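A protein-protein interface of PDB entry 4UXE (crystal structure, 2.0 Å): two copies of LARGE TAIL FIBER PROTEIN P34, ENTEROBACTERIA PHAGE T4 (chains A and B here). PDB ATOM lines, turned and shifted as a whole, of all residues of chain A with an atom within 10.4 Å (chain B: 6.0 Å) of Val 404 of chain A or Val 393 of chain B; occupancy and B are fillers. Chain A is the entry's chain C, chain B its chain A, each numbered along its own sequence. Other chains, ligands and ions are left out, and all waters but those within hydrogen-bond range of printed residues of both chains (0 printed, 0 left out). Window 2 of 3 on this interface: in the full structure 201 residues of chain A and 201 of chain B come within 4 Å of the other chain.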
ATOM      1  N   LEU A 382      39.512 -26.996 -24.328  1.00  0.00           N
ATOM      2  CA  LEU A 382      38.553 -28.054 -24.036  1.00  0.00           C
ATOM      3  C   LEU A 382      37.145 -27.560 -24.345  1.00  0.00           C
ATOM      4  O   LEU A 382      36.814 -26.389 -24.099  1.00  0.00           O
ATOM      5  CB  LEU A 382      38.644 -28.454 -22.555  1.00  0.00           C
ATOM      6  CG  LEU A 382      37.687 -29.507 -21.983  1.00  0.00           C
ATOM      7  CD1 LEU A 382      37.926 -30.880 -22.652  1.00  0.00           C
ATOM      8  CD2 LEU A 382      37.865 -29.580 -20.453  1.00  0.00           C
ATOM      9  N   THR A 383      36.324 -28.472 -24.867  1.00  0.00           N
ATOM     10  CA  THR A 383      34.908 -28.227 -25.078  1.00  0.00           C
ATOM     11  C   THR A 383      34.067 -29.187 -24.209  1.00  0.00           C
ATOM     12  O   THR A 383      34.261 -30.413 -24.231  1.00  0.00           O
ATOM     13  CB  THR A 383      34.541 -28.384 -26.563  1.00  0.00           C
ATOM     14  OG1 THR A 383      35.292 -27.436 -27.352  1.00  0.00           O
ATOM     15  CG2 THR A 383      33.029 -28.158 -26.778  1.00  0.00           C
ATOM     16  N   ILE A 384      33.132 -28.616 -23.451  1.00  0.00           N
ATOM     17  CA  ILE A 384      32.262 -29.380 -22.567  1.00  0.00           C
ATOM     18  C   ILE A 384      30.821 -29.190 -23.052  1.00  0.00           C
ATOM     19  O   ILE A 384      30.326 -28.048 -23.136  1.00  0.00           O
ATOM     20  CB  ILE A 384      32.419 -28.950 -21.098  1.00  0.00           C
ATOM     21  CG1 ILE A 384      33.860 -29.237 -20.596  1.00  0.00           C
ATOM     22  CG2 ILE A 384      31.372 -29.667 -20.248  1.00  0.00           C
ATOM     23  CD1 ILE A 384      34.221 -28.599 -19.252  1.00  0.00           C
ATOM     24  N   ARG A 385      30.166 -30.300 -23.394  1.00  0.00           N
ATOM     25  CA  ARG A 385      28.845 -30.245 -24.004  1.00  0.00           C
ATOM     26  C   ARG A 385      27.774 -29.920 -22.969  1.00  0.00           C
ATOM     27  O   ARG A 385      26.917 -29.062 -23.220  1.00  0.00           O
ATOM     28  CB  ARG A 385      28.530 -31.550 -24.753  1.00  0.00           C
ATOM     29  CG  ARG A 385      27.257 -31.478 -25.601  1.00  0.00           C
ATOM     30  CD  ARG A 385      26.852 -32.845 -26.191  1.00  0.00           C
ATOM     31  NE  ARG A 385      26.572 -33.804 -25.131  1.00  0.00           N
ATOM     32  CZ  ARG A 385      26.487 -35.123 -25.280  1.00  0.00           C
ATOM     33  NH1 ARG A 385      26.635 -35.689 -26.472  1.00  0.00           N
ATOM     34  NH2 ARG A 385      26.246 -35.877 -24.213  1.00  0.00           N
ATOM     35  N   ASP A 386      27.852 -30.553 -21.796  1.00  0.00           N
ATOM     36  CA  ASP A 386      26.743 -30.558 -20.837  1.00  0.00           C
ATOM     37  C   ASP A 386      26.918 -29.697 -19.585  1.00  0.00           C
ATOM     38  O   ASP A 386      26.133 -28.778 -19.366  1.00  0.00           O
ATOM     39  CB  ASP A 386      26.349 -31.997 -20.469  1.00  0.00           C
ATOM     40  CG  ASP A 386      25.942 -32.802 -21.697  1.00  0.00           C
ATOM     41  OD1 ASP A 386      25.288 -32.206 -22.571  1.00  0.00           O
ATOM     42  OD2 ASP A 386      26.307 -33.991 -21.824  1.00  0.00           O
ATOM     43  N   PHE A 387      27.921 -29.986 -18.762  1.00  0.00           N
ATOM     44  CA  PHE A 387      28.201 -29.130 -17.615  1.00  0.00           C
ATOM     45  C   PHE A 387      29.641 -29.241 -17.140  1.00  0.00           C
ATOM     46  O   PHE A 387      30.294 -30.262 -17.329  1.00  0.00           O
ATOM     47  CB  PHE A 387      27.241 -29.394 -16.445  1.00  0.00           C
ATOM     48  CG  PHE A 387      27.397 -30.733 -15.812  1.00  0.00           C
ATOM     49  CD1 PHE A 387      28.309 -30.929 -14.769  1.00  0.00           C
ATOM     50  CD2 PHE A 387      26.613 -31.807 -16.237  1.00  0.00           C
ATOM     51  CE1 PHE A 387      28.458 -32.182 -14.168  1.00  0.00           C
ATOM     52  CE2 PHE A 387      26.745 -33.050 -15.640  1.00  0.00           C
ATOM     53  CZ  PHE A 387      27.669 -33.242 -14.602  1.00  0.00           C
ATOM     54  N   LEU A 388      30.114 -28.165 -16.528  1.00  0.00           N
ATOM     55  CA  LEU A 388      31.360 -28.166 -15.790  1.00  0.00           C
ATOM     56  C   LEU A 388      30.994 -27.980 -14.326  1.00  0.00           C
ATOM     57  O   LEU A 388      30.272 -27.041 -13.973  1.00  0.00           O
ATOM     58  CB  LEU A 388      32.251 -27.009 -16.279  1.00  0.00           C
ATOM     59  CG  LEU A 388      33.476 -26.743 -15.377  1.00  0.00           C
ATOM     60  CD1 LEU A 388      34.455 -27.914 -15.431  1.00  0.00           C
ATOM     61  CD2 LEU A 388      34.160 -25.431 -15.807  1.00  0.00           C
ATOM     62  N   ILE A 390      32.368 -27.229 -10.570  1.00  0.00           N
ATOM     63  CA  ILE A 390      33.483 -26.816  -9.705  1.00  0.00           C
ATOM     64  C   ILE A 390      33.001 -26.911  -8.275  1.00  0.00           C
ATOM     65  O   ILE A 390      32.085 -26.184  -7.878  1.00  0.00           O
ATOM     66  CB  ILE A 390      33.932 -25.357  -9.998  1.00  0.00           C
ATOM     67  CG1 ILE A 390      34.075 -25.104 -11.505  1.00  0.00           C
ATOM     68  CG2 ILE A 390      35.211 -24.976  -9.179  1.00  0.00           C
ATOM     69  CD1 ILE A 390      35.238 -25.741 -12.128  1.00  0.00           C
ATOM     70  N   VAL A 393      29.095 -26.648  -7.493  1.00  0.00           N
ATOM     71  CA  VAL A 393      28.397 -25.755  -8.408  1.00  0.00           C
ATOM     72  C   VAL A 393      28.534 -26.238  -9.855  1.00  0.00           C
ATOM     73  O   VAL A 393      29.652 -26.395 -10.372  1.00  0.00           O
ATOM     74  CB  VAL A 393      28.947 -24.305  -8.297  1.00  0.00           C
ATOM     75  CG1 VAL A 393      28.360 -23.402  -9.372  1.00  0.00           C
ATOM     76  CG2 VAL A 393      28.682 -23.738  -6.907  1.00  0.00           C
ATOM     77  N   ARG A 394      27.400 -26.467 -10.506  1.00  0.00           N
ATOM     78  CA  ARG A 394      27.384 -26.752 -11.942  1.00  0.00           C
ATOM     79  C   ARG A 394      27.358 -25.467 -12.724  1.00  0.00           C
ATOM     80  O   ARG A 394      26.535 -24.594 -12.459  1.00  0.00           O
ATOM     81  CB  ARG A 394      26.156 -27.553 -12.348  1.00  0.00           C
ATOM     82  CG  ARG A 394      26.108 -28.949 -11.880  1.00  0.00           C
ATOM     83  CD  ARG A 394      25.155 -29.717 -12.794  1.00  0.00           C
ATOM     84  NE  ARG A 394      24.407 -30.742 -12.072  1.00  0.00           N
ATOM     85  CZ  ARG A 394      24.920 -31.862 -11.551  1.00  0.00           C
ATOM     86  NH1 ARG A 394      26.221 -32.148 -11.635  1.00  0.00           N
ATOM     87  NH2 ARG A 394      24.112 -32.708 -10.918  1.00  0.00           N
ATOM     88  N   ILE A 395      28.254 -25.358 -13.691  1.00  0.00           N
ATOM     89  CA  ILE A 395      28.276 -24.258 -14.633  1.00  0.00           C
ATOM     90  C   ILE A 395      27.703 -24.819 -15.930  1.00  0.00           C
ATOM     91  O   ILE A 395      28.284 -25.719 -16.555  1.00  0.00           O
ATOM     92  CB  ILE A 395      29.698 -23.698 -14.840  1.00  0.00           C
ATOM     93  CG1 ILE A 395      30.275 -23.221 -13.500  1.00  0.00           C
ATOM     94  CG2 ILE A 395      29.685 -22.585 -15.883  1.00  0.00           C
ATOM     95  CD1 ILE A 395      31.782 -23.007 -13.484  1.00  0.00           C
ATOM     96  N   VAL A 396      26.533 -24.317 -16.309  1.00  0.00           N
ATOM     97  CA  VAL A 396      25.839 -24.823 -17.487  1.00  0.00           C
ATOM     98  C   VAL A 396      25.573 -23.648 -18.434  1.00  0.00           C
ATOM     99  O   VAL A 396      25.722 -22.489 -18.025  1.00  0.00           O
ATOM    100  CB  VAL A 396      24.538 -25.564 -17.100  1.00  0.00           C
ATOM    101  CG1 VAL A 396      24.821 -26.637 -16.065  1.00  0.00           C
ATOM    102  CG2 VAL A 396      23.503 -24.584 -16.563  1.00  0.00           C
ATOM    103  N   PRO A 397      25.222 -23.932 -19.705  1.00  0.00           N
ATOM    104  CA  PRO A 397      24.969 -22.817 -20.626  1.00  0.00           C
ATOM    105  C   PRO A 397      23.597 -22.169 -20.395  1.00  0.00           C
ATOM    106  O   PRO A 397      22.606 -22.876 -20.153  1.00  0.00           O
ATOM    107  CB  PRO A 397      25.031 -23.473 -22.015  1.00  0.00           C
ATOM    108  CG  PRO A 397      25.490 -24.900 -21.793  1.00  0.00           C
ATOM    109  CD  PRO A 397      25.131 -25.238 -20.386  1.00  0.00           C
ATOM    110  N   ASP A 398      23.567 -20.834 -20.442  1.00  0.00           N
ATOM    111  CA  ASP A 398      22.321 -20.056 -20.356  1.00  0.00           C
ATOM    112  C   ASP A 398      22.071 -19.246 -21.644  1.00  0.00           C
ATOM    113  O   ASP A 398      22.657 -18.161 -21.826  1.00  0.00           O
ATOM    114  CB  ASP A 398      22.336 -19.125 -19.131  1.00  0.00           C
ATOM    115  CG  ASP A 398      20.991 -18.423 -18.901  1.00  0.00           C
ATOM    116  OD1 ASP A 398      19.930 -19.018 -19.233  1.00  0.00           O
ATOM    117  OD2 ASP A 398      21.005 -17.282 -18.376  1.00  0.00           O
ATOM    118  N   PRO A 399      21.213 -19.777 -22.543  1.00  0.00           N
ATOM    119  CA  PRO A 399      20.845 -19.103 -23.810  1.00  0.00           C
ATOM    120  C   PRO A 399      20.239 -17.693 -23.643  1.00  0.00           C
ATOM    121  O   PRO A 399      20.594 -16.771 -24.396  1.00  0.00           O
ATOM    122  CB  PRO A 399      19.829 -20.069 -24.453  1.00  0.00           C
ATOM    123  CG  PRO A 399      19.462 -21.060 -23.368  1.00  0.00           C
ATOM    124  CD  PRO A 399      20.640 -21.133 -22.456  1.00  0.00           C
ATOM    125  N   VAL A 400      19.369 -17.542 -22.641  1.00  0.00           N
ATOM    126  CA  VAL A 400      18.616 -16.305 -22.392  1.00  0.00           C
ATOM    127  C   VAL A 400      19.475 -15.044 -22.132  1.00  0.00           C
ATOM    128  O   VAL A 400      19.044 -13.932 -22.454  1.00  0.00           O
ATOM    129  CB  VAL A 400      17.533 -16.490 -21.274  1.00  0.00           C
ATOM    130  CG1 VAL A 400      16.789 -17.830 -21.451  1.00  0.00           C
ATOM    131  CG2 VAL A 400      18.135 -16.371 -19.870  1.00  0.00           C
ATOM    132  N   ASN A 401      20.674 -15.208 -21.569  1.00  0.00           N
ATOM    133  CA  ASN A 401      21.579 -14.065 -21.353  1.00  0.00           C
ATOM    134  C   ASN A 401      22.855 -14.130 -22.207  1.00  0.00           C
ATOM    135  O   ASN A 401      23.703 -13.224 -22.142  1.00  0.00           O
ATOM    136  CB  ASN A 401      21.940 -13.902 -19.863  1.00  0.00           C
ATOM    137  CG  ASN A 401      20.713 -13.683 -18.964  1.00  0.00           C
ATOM    138  OD1 ASN A 401      19.634 -13.301 -19.429  1.00  0.00           O
ATOM    139  ND2 ASN A 401      20.887 -13.922 -17.663  1.00  0.00           N
ATOM    140  N   LYS A 402      22.970 -15.199 -23.004  1.00  0.00           N
ATOM    141  CA  LYS A 402      24.159 -15.493 -23.829  1.00  0.00           C
ATOM    142  C   LYS A 402      25.462 -15.635 -23.015  1.00  0.00           C
ATOM    143  O   LYS A 402      26.546 -15.240 -23.472  1.00  0.00           O
ATOM    144  CB  LYS A 402      24.316 -14.476 -24.974  1.00  0.00           C
ATOM    145  CG  LYS A 402      23.117 -14.399 -25.916  1.00  0.00           C
ATOM    146  CD  LYS A 402      23.126 -13.094 -26.712  1.00  0.00           C
ATOM    147  CE  LYS A 402      21.741 -12.774 -27.266  1.00  0.00           C
ATOM    148  NZ  LYS A 402      21.724 -11.476 -28.006  1.00  0.00           N
ATOM    149  N   THR A 403      25.331 -16.184 -21.802  1.00  0.00           N
ATOM    150  CA  THR A 403      26.473 -16.574 -20.962  1.00  0.00           C
ATOM    151  C   THR A 403      26.185 -17.916 -20.272  1.00  0.00           C
ATOM    152  O   THR A 403      25.442 -18.760 -20.793  1.00  0.00           O
ATOM    153  CB  THR A 403      26.870 -15.491 -19.888  1.00  0.00           C
ATOM    154  OG1 THR A 403      25.729 -15.131 -19.101  1.00  0.00           O
ATOM    155  CG2 THR A 403      27.487 -14.238 -20.524  1.00  0.00           C
ATOM    156  N   VAL A 404      26.783 -18.104 -19.101  1.00  0.00           N
ATOM    157  CA  VAL A 404      26.610 -19.322 -18.320  1.00  0.00           C
ATOM    158  C   VAL A 404      25.803 -19.035 -17.066  1.00  0.00           C
ATOM    159  O   VAL A 404      25.909 -17.947 -16.491  1.00  0.00           O
ATOM    160  CB  VAL A 404      27.978 -19.941 -17.899  1.00  0.00           C
ATOM    161  CG1 VAL A 404      28.748 -20.416 -19.110  1.00  0.00           C
ATOM    162  CG2 VAL A 404      28.817 -18.959 -17.073  1.00  0.00           C
ATOM    163  N   LYS A 405      25.001 -20.007 -16.636  1.00  0.00           N
ATOM    164  CA  LYS A 405      24.395 -19.922 -15.311  1.00  0.00           C
ATOM    165  C   LYS A 405      25.033 -20.907 -14.320  1.00  0.00           C
ATOM    166  O   LYS A 405      25.475 -21.996 -14.705  1.00  0.00           O
ATOM    167  CB  LYS A 405      22.867 -20.053 -15.367  1.00  0.00           C
ATOM    168  CG  LYS A 405      22.325 -21.313 -16.007  1.00  0.00           C
ATOM    169  CD  LYS A 405      20.839 -21.144 -16.305  1.00  0.00           C
ATOM    170  CE  LYS A 405      20.305 -22.206 -17.254  1.00  0.00           C
ATOM    171  NZ  LYS A 405      19.890 -23.447 -16.538  1.00  0.00           N
ATOM    172  N   PHE A 406      25.085 -20.503 -13.052  1.00  0.00           N
ATOM    173  CA  PHE A 406      25.561 -21.366 -11.982  1.00  0.00           C
ATOM    174  C   PHE A 406      24.390 -22.058 -11.294  1.00  0.00           C
ATOM    175  O   PHE A 406      23.323 -21.472 -11.136  1.00  0.00           O
ATOM    176  CB  PHE A 406      26.381 -20.569 -10.963  1.00  0.00           C
ATOM    177  CG  PHE A 406      27.495 -19.750 -11.568  1.00  0.00           C
ATOM    178  CD1 PHE A 406      28.288 -20.258 -12.593  1.00  0.00           C
ATOM    179  CD2 PHE A 406      27.772 -18.472 -11.084  1.00  0.00           C
ATOM    180  CE1 PHE A 406      29.319 -19.503 -13.149  1.00  0.00           C
ATOM    181  CE2 PHE A 406      28.810 -17.703 -11.632  1.00  0.00           C
ATOM    182  CZ  PHE A 406      29.583 -18.227 -12.667  1.00  0.00           C
ATOM    183  N   GLU A 407      24.581 -23.311 -10.905  1.00  0.00           N
ATOM    184  CA  GLU A 407      23.559 -24.049 -10.174  1.00  0.00           C
ATOM    185  C   GLU A 407      24.195 -24.801  -9.022  1.00  0.00           C
ATOM    186  O   GLU A 407      25.087 -25.623  -9.234  1.00  0.00           O
ATOM    187  CB  GLU A 407      22.828 -25.045 -11.083  1.00  0.00           C
ATOM    188  CG  GLU A 407      22.274 -24.457 -12.378  1.00  0.00           C
ATOM    189  CD  GLU A 407      21.528 -25.485 -13.218  1.00  0.00           C
ATOM    190  OE1 GLU A 407      21.782 -26.707 -13.064  1.00  0.00           O
ATOM    191  OE2 GLU A 407      20.685 -25.062 -14.041  1.00  0.00           O
ATOM    192  N   LEU B 388      38.077 -22.361 -23.047  1.00  0.00           N
ATOM    193  CA  LEU B 388      37.156 -23.381 -22.555  1.00  0.00           C
ATOM    194  C   LEU B 388      35.776 -23.050 -23.115  1.00  0.00           C
ATOM    195  O   LEU B 388      35.263 -21.938 -22.931  1.00  0.00           O
ATOM    196  CB  LEU B 388      37.105 -23.382 -21.030  1.00  0.00           C
ATOM    197  CG  LEU B 388      35.996 -24.227 -20.398  1.00  0.00           C
ATOM    198  CD1 LEU B 388      36.317 -25.722 -20.535  1.00  0.00           C
ATOM    199  CD2 LEU B 388      35.809 -23.824 -18.942  1.00  0.00           C
ATOM    200  N   ARG B 389      35.176 -24.004 -23.803  1.00  0.00           N
ATOM    201  CA  ARG B 389      33.831 -23.828 -24.310  1.00  0.00           C
ATOM    202  C   ARG B 389      32.879 -24.720 -23.512  1.00  0.00           C
ATOM    203  O   ARG B 389      33.186 -25.913 -23.272  1.00  0.00           O
ATOM    204  CB  ARG B 389      33.812 -24.147 -25.801  1.00  0.00           C
ATOM    205  CG  ARG B 389      32.460 -23.984 -26.430  1.00  0.00           C
ATOM    206  CD  ARG B 389      32.514 -24.178 -27.919  1.00  0.00           C
ATOM    207  NE  ARG B 389      31.152 -24.271 -28.434  1.00  0.00           N
ATOM    208  CZ  ARG B 389      30.833 -24.523 -29.698  1.00  0.00           C
ATOM    209  NH1 ARG B 389      31.783 -24.725 -30.612  1.00  0.00           N
ATOM    210  NH2 ARG B 389      29.553 -24.578 -30.046  1.00  0.00           N
ATOM    211  N   ILE B 390      31.769 -24.136 -23.054  1.00  0.00           N
ATOM    212  CA  ILE B 390      30.677 -24.887 -22.396  1.00  0.00           C
ATOM    213  C   ILE B 390      29.386 -24.653 -23.189  1.00  0.00           C
ATOM    214  O   ILE B 390      28.845 -23.533 -23.194  1.00  0.00           O
ATOM    215  CB  ILE B 390      30.463 -24.493 -20.919  1.00  0.00           C
ATOM    216  CG1 ILE B 390      31.758 -24.667 -20.106  1.00  0.00           C
ATOM    217  CG2 ILE B 390      29.313 -25.321 -20.294  1.00  0.00           C
ATOM    218  CD1 ILE B 390      31.716 -24.052 -18.732  1.00  0.00           C
ATOM    219  N   GLY B 391      28.916 -25.691 -23.879  1.00  0.00           N
ATOM    220  CA  GLY B 391      27.784 -25.550 -24.797  1.00  0.00           C
ATOM    221  C   GLY B 391      28.196 -24.562 -25.872  1.00  0.00           C
ATOM    222  O   GLY B 391      29.218 -24.756 -26.534  1.00  0.00           O
ATOM    223  N   ASN B 392      27.433 -23.482 -26.021  1.00  0.00           N
ATOM    224  CA  ASN B 392      27.744 -22.479 -27.043  1.00  0.00           C
ATOM    225  C   ASN B 392      28.509 -21.267 -26.544  1.00  0.00           C
ATOM    226  O   ASN B 392      28.733 -20.340 -27.307  1.00  0.00           O
ATOM    227  CB  ASN B 392      26.475 -22.020 -27.775  1.00  0.00           C
ATOM    228  CG  ASN B 392      25.836 -23.138 -28.566  1.00  0.00           C
ATOM    229  OD1 ASN B 392      26.450 -23.700 -29.483  1.00  0.00           O
ATOM    230  ND2 ASN B 392      24.605 -23.494 -28.197  1.00  0.00           N
ATOM    231  N   VAL B 393      28.916 -21.255 -25.281  1.00  0.00           N
ATOM    232  CA  VAL B 393      29.732 -20.132 -24.812  1.00  0.00           C
ATOM    233  C   VAL B 393      31.222 -20.487 -24.675  1.00  0.00           C
ATOM    234  O   VAL B 393      31.577 -21.458 -23.998  1.00  0.00           O
ATOM    235  CB  VAL B 393      29.123 -19.417 -23.566  1.00  0.00           C
ATOM    236  CG1 VAL B 393      28.750 -20.393 -22.479  1.00  0.00           C
ATOM    237  CG2 VAL B 393      30.063 -18.322 -23.038  1.00  0.00           C
ATOM    238  N   ARG B 394      32.067 -19.729 -25.385  1.00  0.00           N
ATOM    239  CA  ARG B 394      33.519 -19.764 -25.215  1.00  0.00           C
ATOM    240  C   ARG B 394      33.924 -18.845 -24.088  1.00  0.00           C
ATOM    241  O   ARG B 394      33.487 -17.687 -24.035  1.00  0.00           O
ATOM    242  CB  ARG B 394      34.245 -19.287 -26.466  1.00  0.00           C
ATOM    243  CG  ARG B 394      34.372 -20.301 -27.575  1.00  0.00           C
ATOM    244  CD  ARG B 394      34.690 -19.601 -28.893  1.00  0.00           C
ATOM    245  NE  ARG B 394      35.983 -18.926 -28.851  1.00  0.00           N
ATOM    246  CZ  ARG B 394      37.124 -19.490 -29.234  1.00  0.00           C
ATOM    247  NH1 ARG B 394      37.119 -20.739 -29.692  1.00  0.00           N
ATOM    248  NH2 ARG B 394      38.267 -18.807 -29.165  1.00  0.00           N
ATOM    249  N   ILE B 395      34.755 -19.361 -23.192  1.00  0.00           N
ATOM    250  CA  ILE B 395      35.363 -18.577 -22.130  1.00  0.00           C
ATOM    251  C   ILE B 395      36.862 -18.405 -22.445  1.00  0.00           C
ATOM    252  O   ILE B 395      37.630 -19.376 -22.419  1.00  0.00           O
ATOM    253  CB  ILE B 395      35.150 -19.246 -20.766  1.00  0.00           C
ATOM    254  CG1 ILE B 395      33.668 -19.589 -20.590  1.00  0.00           C
ATOM    255  CG2 ILE B 395      35.689 -18.351 -19.648  1.00  0.00           C
ATOM    256  CD1 ILE B 395      33.364 -20.606 -19.515  1.00  0.00           C
ATOM    257  N   PHE B 406      33.383 -13.736 -22.075  1.00  0.00           N
ATOM    258  CA  PHE B 406      32.395 -14.706 -22.553  1.00  0.00           C
ATOM    259  C   PHE B 406      32.026 -14.382 -23.995  1.00  0.00           C
ATOM    260  O   PHE B 406      32.135 -13.232 -24.429  1.00  0.00           O
ATOM    261  CB  PHE B 406      31.174 -14.733 -21.642  1.00  0.00           C
ATOM    262  CG  PHE B 406      31.472 -15.248 -20.269  1.00  0.00           C
ATOM    263  CD1 PHE B 406      32.336 -14.562 -19.425  1.00  0.00           C
ATOM    264  CD2 PHE B 406      30.906 -16.432 -19.822  1.00  0.00           C
ATOM    265  CE1 PHE B 406      32.623 -15.046 -18.153  1.00  0.00           C
ATOM    266  CE2 PHE B 406      31.185 -16.926 -18.548  1.00  0.00           C
ATOM    267  CZ  PHE B 406      32.040 -16.233 -17.713  1.00  0.00           C
ATOM    268  N   GLU B 407      31.598 -15.394 -24.740  1.00  0.00           N
ATOM    269  CA  GLU B 407      31.633 -15.317 -26.195  1.00  0.00           C
ATOM    270  C   GLU B 407      30.714 -16.374 -26.826  1.00  0.00           C
ATOM    271  O   GLU B 407      31.138 -17.507 -27.085  1.00  0.00           O
ATOM    272  CB  GLU B 407      33.083 -15.526 -26.643  1.00  0.00           C
ATOM    273  CG  GLU B 407      33.536 -14.745 -27.848  1.00  0.00           C
ATOM    274  CD  GLU B 407      35.051 -14.586 -27.872  1.00  0.00           C
ATOM    275  OE1 GLU B 407      35.566 -13.678 -27.179  1.00  0.00           O
ATOM    276  OE2 GLU B 407      35.727 -15.382 -28.566  1.00  0.00           O
ATOM    277  N   TRP B 408      29.459 -15.999 -27.071  1.00  0.00           N
ATOM    278  CA  TRP B 408      28.475 -16.922 -27.626  1.00  0.00           C
ATOM    279  C   TRP B 408      28.858 -17.293 -29.057  1.00  0.00           C
ATOM    280  O   TRP B 408      29.229 -16.420 -29.842  1.00  0.00           O
ATOM    281  CB  TRP B 408      27.071 -16.312 -27.561  1.00  0.00           C
ATOM    282  CG  TRP B 408      25.957 -17.309 -27.728  1.00  0.00           C
ATOM    283  CD1 TRP B 408      25.295 -17.610 -28.884  1.00  0.00           C
ATOM    284  CD2 TRP B 408      25.372 -18.133 -26.707  1.00  0.00           C
ATOM    285  NE1 TRP B 408      24.338 -18.568 -28.649  1.00  0.00           N
ATOM    286  CE2 TRP B 408      24.363 -18.910 -27.323  1.00  0.00           C
ATOM    287  CE3 TRP B 408      25.608 -18.298 -25.332  1.00  0.00           C
ATOM    288  CZ2 TRP B 408      23.586 -19.838 -26.612  1.00  0.00           C
ATOM    289  CZ3 TRP B 408      24.830 -19.223 -24.622  1.00  0.00           C
ATOM    290  CH2 TRP B 408      23.835 -19.982 -25.269  1.00  0.00           C
ATOM    291  N   VAL B 409      28.802 -18.590 -29.370  1.00  0.00           N
ATOM    292  CA  VAL B 409      29.097 -19.119 -30.711  1.00  0.00           C
ATOM    293  C   VAL B 409      28.023 -20.114 -31.154  1.00  0.00           C
ATOM    294  O   VAL B 409      26.943 -19.723 -31.593  1.00  0.00           O
ATOM    295  CB  VAL B 409      30.513 -19.780 -30.798  1.00  0.00           C
ATOM    296  CG1 VAL B 409      30.702 -20.849 -29.734  1.00  0.00           C
ATOM    297  CG2 VAL B 409      30.765 -20.368 -32.190  1.00  0.00           C
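Of the 12 printed residues of chain B, 7 touch a printed residue of chain A.
Hydrophobic or aromatic side chains of chain A that line the printed part of chain B: Ile 384, Leu 388, Ile 395, Pro 397 and Val 404.
The guanidinium group (NE) of Arg 389 of chain B lies within hydrogen-bond range of the backbone carbonyl oxygen (O) of Gly 391 of chain B (2.8 Å).
N of Ile 395 of chain A lies within hydrogen-bond range of O of Leu 388 of chain A (2.6 Å).
The backbone NH of Asp 398 of chain A lies within hydrogen-bond range of the backbone carbonyl oxygen of Thr 403 of chain A.
The side-chain carboxylate of Asp 398 of chain A is in hydrogen-bond range of the side-chain amide nitrogen of Asn 401 of chain A, 3.4 Å away.
The backbone NH (N) of Ile 395 of chain B sits at hydrogen-bond distance from the backbone carbonyl oxygen (O) of Leu 388 of chain B (2.6 Å).
NH2 of Arg 389 of chain B lies within hydrogen-bond range of OD1 of Asn 392 of chain B (3.3 Å).
Val 404 of chain A touches just these residues of chain B: Val 393 and Phe 406.
Val 393 of chain B touches just one residue of chain A: Val 404 (3.4 Å).
Ile 390 of chain B touches just these residues of chain A: Ile 384, Leu 388, Ile 395 and Pro 397.
Of chain A, only Ile 384 (2.8 Å), Arg 385 (3.9 Å) and Pro 397 (3.8 Å) come within 4 Å of Gly 391 of chain B.
No residue of chain A comes within 4 Å of Asn 392 of chain B.
Phe 406 of chain B touches just these residues of chain A: Thr 403 and Val 404.
Of chain A, only Asp 398, Pro 399, Lys 402 and Thr 403 come within 4 Å of Trp 408 of chain B.
Printed residues of chain A within 4 Å of Arg 389 of chain B: Leu 382 (2.9 Å), Thr 383 (3.4 Å) and Ile 384 (2.7 Å).
Of the printed residues of chain B, Ile 384 of chain A touches Leu 388, Arg 389, Ile 390 and Gly 391.
Of the printed residues of chain B, Pro 399 of chain A touches Trp 408.
Of the printed residues of chain B, Thr 403 of chain A touches Phe 406 (3.9 Å) and Trp 408 (3.9 Å).
Ile 395 of chain B touches none of the printed residues of chain A.
The nearest residue of chain A that does not touch Val 393 of chain B is Thr 403 of chain A (4.1 Å).
The nearest printed residue of chain B that does not touch Leu 388 of chain A is Ile 395 of chain B (6.1 Å).
Leu 388 of chain A touches its own counterpart, Leu 388 of chain B.
Leu 388 of chain A touches Ile 390 of chain B, but with the chains exchanged Ile 390 of chain A does not touch Leu 388 of chain B (7.1 Å).
Ile 395 of chain A touches Ile 390 of chain B, but with the chains exchanged Ile 390 of chain A does not touch Ile 395 of chain B (9.2 Å).
Positions printed for both chains: 388, 390, 393, 394, 395, 406 and 407.
Of the 20 pairs that touch across the chains among the printed residues, 1 has its exchanged pair printed and touching as well.
Thr 383 of chain A touches Arg 389 of chain B (CA to O, 3.4 Å).
Ile 384 of chain A touches Leu 388 of chain B.
Leu 388 of chain A touches Leu 388 of chain B (CD2 to CD2, 3.9 Å).
O of Ile 390 of chain B touches CG of Pro 397 of chain A, 3.9 Å away.
Gly 391 of chain B touches Pro 397 of chain A.
Trp 408 of chain B touches Asp 398 of chain A (CZ3 to O, 3.7 Å).
Pro 399 of chain A touches Trp 408 of chain B.
O of Thr 403 of chain A touches CZ3 of Trp 408 of chain B, 3.9 Å away.
CG1 of Val 404 of chain A touches CG1 of Val 393 of chain B (3.4 Å).
Phe 406 of chain B touches Val 404 of chain A.
The backbone carbonyl oxygen (O) of Ile 384 of chain A sits at hydrogen-bond distance from the backbone NH (N) of Gly 391 of chain B (2.8 Å).
The backbone NH (N) of Ile 384 of chain A lies within hydrogen-bond range of the backbone carbonyl oxygen (O) of Arg 389 of chain B (2.7 Å).
The backbone NH (N) of Arg 389 of chain B lies within hydrogen-bond range of the backbone carbonyl oxygen (O) of Leu 382 of chain A, 2.9 Å away.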
